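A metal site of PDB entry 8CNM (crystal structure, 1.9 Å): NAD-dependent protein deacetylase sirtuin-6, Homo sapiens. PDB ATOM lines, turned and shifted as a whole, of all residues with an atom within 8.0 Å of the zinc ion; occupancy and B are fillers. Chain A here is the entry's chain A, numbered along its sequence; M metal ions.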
ATOM      1  N   GLU A 134      27.914  15.840  26.276  1.00  0.00           N
ATOM      2  CA  GLU A 134      27.325  16.247  27.577  1.00  0.00           C
ATOM      3  C   GLU A 134      25.793  16.275  27.471  1.00  0.00           C
ATOM      4  O   GLU A 134      25.294  16.813  26.471  1.00  0.00           O
ATOM      5  CB  GLU A 134      27.898  17.610  27.959  1.00  0.00           C
ATOM      6  CG  GLU A 134      27.297  18.215  29.219  1.00  0.00           C
ATOM      7  CD  GLU A 134      27.995  19.510  29.617  1.00  0.00           C
ATOM      8  OE1 GLU A 134      29.204  19.478  29.877  1.00  0.00           O
ATOM      9  OE2 GLU A 134      27.324  20.545  29.630  1.00  0.00           O
ATOM     10  N   CYS A 135      25.103  15.790  28.493  1.00  0.00           N
ATOM     11  CA  CYS A 135      23.624  15.821  28.535  1.00  0.00           C
ATOM     12  C   CYS A 135      23.161  17.229  28.880  1.00  0.00           C
ATOM     13  O   CYS A 135      23.643  17.783  29.864  1.00  0.00           O
ATOM     14  CB  CYS A 135      23.134  14.902  29.642  1.00  0.00           C
ATOM     15  SG  CYS A 135      21.342  14.815  29.833  1.00  0.00           S
ATOM     16  N   ALA A 136      22.242  17.774  28.096  1.00  0.00           N
ATOM     17  CA  ALA A 136      21.684  19.106  28.399  1.00  0.00           C
ATOM     18  C   ALA A 136      20.939  19.097  29.738  1.00  0.00           C
ATOM     19  O   ALA A 136      21.006  20.104  30.443  1.00  0.00           O
ATOM     20  CB  ALA A 136      20.781  19.500  27.268  1.00  0.00           C
ATOM     21  N   LYS A 137      20.196  18.025  30.024  1.00  0.00           N
ATOM     22  CA  LYS A 137      19.382  17.960  31.262  1.00  0.00           C
ATOM     23  C   LYS A 137      20.187  17.767  32.549  1.00  0.00           C
ATOM     24  O   LYS A 137      20.024  18.584  33.449  1.00  0.00           O
ATOM     25  CB  LYS A 137      18.363  16.823  31.157  1.00  0.00           C
ATOM     26  CG  LYS A 137      17.275  16.969  30.117  1.00  0.00           C
ATOM     27  CD  LYS A 137      16.234  15.889  30.253  1.00  0.00           C
ATOM     28  CE  LYS A 137      15.099  16.001  29.249  1.00  0.00           C
ATOM     29  NZ  LYS A 137      14.192  14.827  29.333  1.00  0.00           N
ATOM     30  N   CYS A 138      21.080  16.768  32.604  1.00  0.00           N
ATOM     31  CA  CYS A 138      21.756  16.437  33.888  1.00  0.00           C
ATOM     32  C   CYS A 138      23.239  16.815  33.882  1.00  0.00           C
ATOM     33  O   CYS A 138      23.890  16.576  34.895  1.00  0.00           O
ATOM     34  CB  CYS A 138      21.577  14.969  34.232  1.00  0.00           C
ATOM     35  SG  CYS A 138      22.540  13.844  33.193  1.00  0.00           S
ATOM     36  N   LYS A 139      23.747  17.326  32.760  1.00  0.00           N
ATOM     37  CA  LYS A 139      25.150  17.792  32.646  1.00  0.00           C
ATOM     38  C   LYS A 139      26.122  16.604  32.699  1.00  0.00           C
ATOM     39  O   LYS A 139      27.317  16.851  32.861  1.00  0.00           O
ATOM     40  CB  LYS A 139      25.456  18.881  33.676  1.00  0.00           C
ATOM     41  CG  LYS A 139      24.474  20.036  33.694  1.00  0.00           C
ATOM     42  CD  LYS A 139      24.287  20.696  32.357  1.00  0.00           C
ATOM     43  CE  LYS A 139      23.304  21.854  32.405  1.00  0.00           C
ATOM     44  NZ  LYS A 139      23.176  22.536  31.090  1.00  0.00           N
ATOM     45  N   THR A 140      25.629  15.384  32.532  1.00  0.00           N
ATOM     46  CA  THR A 140      26.564  14.246  32.653  1.00  0.00           C
ATOM     47  C   THR A 140      27.362  14.143  31.350  1.00  0.00           C
ATOM     48  O   THR A 140      26.754  14.273  30.295  1.00  0.00           O
ATOM     49  CB  THR A 140      25.875  12.938  33.037  1.00  0.00           C
ATOM     50  OG1 THR A 140      25.377  13.037  34.370  1.00  0.00           O
ATOM     51  CG2 THR A 140      26.774  11.732  32.919  1.00  0.00           C
ATOM     52  N   GLN A 141      28.667  13.961  31.457  1.00  0.00           N
ATOM     53  CA  GLN A 141      29.613  13.912  30.316  1.00  0.00           C
ATOM     54  C   GLN A 141      29.927  12.455  29.986  1.00  0.00           C
ATOM     55  O   GLN A 141      29.936  11.599  30.892  1.00  0.00           O
ATOM     56  CB  GLN A 141      30.875  14.696  30.660  1.00  0.00           C
ATOM     57  CG  GLN A 141      30.575  16.193  30.768  1.00  0.00           C
ATOM     58  CD  GLN A 141      31.805  17.059  30.792  1.00  0.00           C
ATOM     59  OE1 GLN A 141      32.849  16.655  31.290  1.00  0.00           O
ATOM     60  NE2 GLN A 141      31.674  18.263  30.250  1.00  0.00           N
ATOM     61  N   TYR A 142      30.167  12.189  28.701  1.00  0.00           N
ATOM     62  CA  TYR A 142      30.499  10.848  28.185  1.00  0.00           C
ATOM     63  C   TYR A 142      31.786  11.010  27.402  1.00  0.00           C
ATOM     64  O   TYR A 142      31.806  11.912  26.565  1.00  0.00           O
ATOM     65  CB  TYR A 142      29.361  10.286  27.332  1.00  0.00           C
ATOM     66  CG  TYR A 142      28.071  10.071  28.077  1.00  0.00           C
ATOM     67  CD1 TYR A 142      27.207  11.131  28.294  1.00  0.00           C
ATOM     68  CD2 TYR A 142      27.714   8.833  28.572  1.00  0.00           C
ATOM     69  CE1 TYR A 142      26.019  10.955  28.986  1.00  0.00           C
ATOM     70  CE2 TYR A 142      26.515   8.628  29.246  1.00  0.00           C
ATOM     71  CZ  TYR A 142      25.665   9.700  29.449  1.00  0.00           C
ATOM     72  OH  TYR A 142      24.489   9.552  30.112  1.00  0.00           O
ATOM     73  N   LEU A 159      21.102   9.825  23.294  1.00  0.00           N
ATOM     74  CA  LEU A 159      20.394  10.249  24.530  1.00  0.00           C
ATOM     75  C   LEU A 159      21.191   9.789  25.749  1.00  0.00           C
ATOM     76  O   LEU A 159      21.970   8.818  25.618  1.00  0.00           O
ATOM     77  CB  LEU A 159      18.972   9.657  24.538  1.00  0.00           C
ATOM     78  CG  LEU A 159      18.064  10.095  23.396  1.00  0.00           C
ATOM     79  CD1 LEU A 159      16.713   9.386  23.495  1.00  0.00           C
ATOM     80  CD2 LEU A 159      17.857  11.597  23.375  1.00  0.00           C
ATOM     81  N   CYS A 160      20.952  10.450  26.897  1.00  0.00           N
ATOM     82  CA  CYS A 160      21.595  10.113  28.188  1.00  0.00           C
ATOM     83  C   CYS A 160      21.138   8.736  28.678  1.00  0.00           C
ATOM     84  O   CYS A 160      19.963   8.417  28.483  1.00  0.00           O
ATOM     85  CB  CYS A 160      21.184  11.137  29.226  1.00  0.00           C
ATOM     86  SG  CYS A 160      22.229  11.278  30.695  1.00  0.00           S
ATOM     87  N   THR A 161      22.015   8.005  29.339  1.00  0.00           N
ATOM     88  CA  THR A 161      21.748   6.620  29.804  1.00  0.00           C
ATOM     89  C   THR A 161      21.831   6.565  31.343  1.00  0.00           C
ATOM     90  O   THR A 161      21.881   5.464  31.879  1.00  0.00           O
ATOM     91  CB  THR A 161      22.699   5.617  29.124  1.00  0.00           C
ATOM     92  OG1 THR A 161      24.048   5.938  29.469  1.00  0.00           O
ATOM     93  CG2 THR A 161      22.562   5.637  27.615  1.00  0.00           C
ATOM     94  N   VAL A 162      21.850   7.720  32.018  1.00  0.00           N
ATOM     95  CA  VAL A 162      21.923   7.787  33.504  1.00  0.00           C
ATOM     96  C   VAL A 162      20.563   7.365  34.083  1.00  0.00           C
ATOM     97  O   VAL A 162      19.536   7.873  33.592  1.00  0.00           O
ATOM     98  CB  VAL A 162      22.335   9.184  34.013  1.00  0.00           C
ATOM     99  CG1 VAL A 162      22.132   9.325  35.513  1.00  0.00           C
ATOM    100  CG2 VAL A 162      23.776   9.516  33.659  1.00  0.00           C
ATOM    101  N   ALA A 163      20.591   6.497  35.102  1.00  0.00           N
ATOM    102  CA  ALA A 163      19.432   5.975  35.867  1.00  0.00           C
ATOM    103  C   ALA A 163      18.605   7.145  36.436  1.00  0.00           C
ATOM    104  O   ALA A 163      19.053   7.696  37.456  1.00  0.00           O
ATOM    105  CB  ALA A 163      19.927   5.074  36.973  1.00  0.00           C
ATOM    106  N   CYS A 171      17.213   9.211  32.356  1.00  0.00           N
ATOM    107  CA  CYS A 171      17.255  10.662  32.027  1.00  0.00           C
ATOM    108  C   CYS A 171      16.855  10.853  30.572  1.00  0.00           C
ATOM    109  O   CYS A 171      16.032  11.728  30.299  1.00  0.00           O
ATOM    110  CB  CYS A 171      18.650  11.215  32.210  1.00  0.00           C
ATOM    111  SG  CYS A 171      18.849  12.910  31.615  1.00  0.00           S
ATOM    112  N   ARG A 172      17.439  10.047  29.690  1.00  0.00           N
ATOM    113  CA  ARG A 172      17.173  10.155  28.226  1.00  0.00           C
ATOM    114  C   ARG A 172      17.360  11.600  27.744  1.00  0.00           C
ATOM    115  O   ARG A 172      16.828  11.963  26.671  1.00  0.00           O
ATOM    116  CB  ARG A 172      15.768   9.633  27.906  1.00  0.00           C
ATOM    117  CG  ARG A 172      15.412   8.311  28.594  1.00  0.00           C
ATOM    118  CD  ARG A 172      14.414   7.458  27.824  1.00  0.00           C
ATOM    119  NE  ARG A 172      13.554   8.257  26.951  1.00  0.00           N
ATOM    120  CZ  ARG A 172      13.546   8.224  25.614  1.00  0.00           C
ATOM    121  NH1 ARG A 172      14.349   7.411  24.952  1.00  0.00           N
ATOM    122  NH2 ARG A 172      12.711   9.007  24.948  1.00  0.00           N
ATOM    123  N   GLY A 173      18.165  12.399  28.459  1.00  0.00           N
ATOM    124  CA  GLY A 173      18.494  13.773  28.047  1.00  0.00           C
ATOM    125  C   GLY A 173      19.201  13.783  26.704  1.00  0.00           C
ATOM    126  O   GLY A 173      19.835  12.759  26.364  1.00  0.00           O
ATOM    127  N   GLU A 174      19.075  14.892  25.970  1.00  0.00           N
ATOM    128  CA  GLU A 174      19.742  15.137  24.660  1.00  0.00           C
ATOM    129  C   GLU A 174      21.247  15.312  24.889  1.00  0.00           C
ATOM    130  O   GLU A 174      21.629  16.238  25.626  1.00  0.00           O
ATOM    131  CB  GLU A 174      19.103  16.365  24.001  1.00  0.00           C
ATOM    132  CG  GLU A 174      19.686  16.760  22.657  1.00  0.00           C
ATOM    133  CD  GLU A 174      18.958  17.890  21.965  1.00  0.00           C
ATOM    134  OE1 GLU A 174      17.860  17.635  21.408  1.00  0.00           O
ATOM    135  OE2 GLU A 174      19.470  19.040  21.982  1.00  0.00           O
ATOM    136  N   LEU A 175      22.076  14.420  24.306  1.00  0.00           N
ATOM    137  CA  LEU A 175      23.553  14.573  24.346  1.00  0.00           C
ATOM    138  C   LEU A 175      23.952  15.619  23.302  1.00  0.00           C
ATOM    139  O   LEU A 175      23.399  15.586  22.181  1.00  0.00           O
ATOM    140  CB  LEU A 175      24.250  13.232  24.070  1.00  0.00           C
ATOM    141  CG  LEU A 175      23.973  12.104  25.075  1.00  0.00           C
ATOM    142  CD1 LEU A 175      25.036  11.023  24.937  1.00  0.00           C
ATOM    143  CD2 LEU A 175      23.903  12.595  26.505  1.00  0.00           C
HETATM  144 ZN    ZN M   1      21.165  13.182  31.470  1.00  0.00          ZN
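The zinc ion is bound by SG of Cys 138, at 2.3 Å. The zinc ion is bound by SG of Cys 160, at 2.3 Å. The side-chain sulfur (SG) of Cys 135 binds the zinc ion, at 2.3 Å. The zinc ion is bound by SG of Cys 171 (2.3 Å).
The side-chain sulfur (SG) of Cys 138 sits close to the side-chain hydroxyl (OG1) of Thr 140 (3.2 Å). SG of Cys 160 sits close to OH of Tyr 142 (2.9 Å). N of Lys 137 sits close to SG of Cys 135 (3.4 Å). The side-chain sulfur of Cys 171 lies close to the backbone NH of Gly 173 (3.3 Å). O of Cys 160 lies within hydrogen-bond range of N of Arg 172 (3.2 Å). The backbone carbonyl oxygen of Thr 140 is in hydrogen-bond range of the backbone NH of Cys 135, 2.9 Å away. N of Cys 171 is in hydrogen-bond range of O of Val 162 (3.0 Å). The backbone carbonyl oxygen of Gly 173 lies within hydrogen-bond range of the backbone NH of Cys 160, 2.6 Å away.
Four residues have an atom within 4 Å of the zinc ion: Cys 135, Cys 138, Cys 160 and Cys 171.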
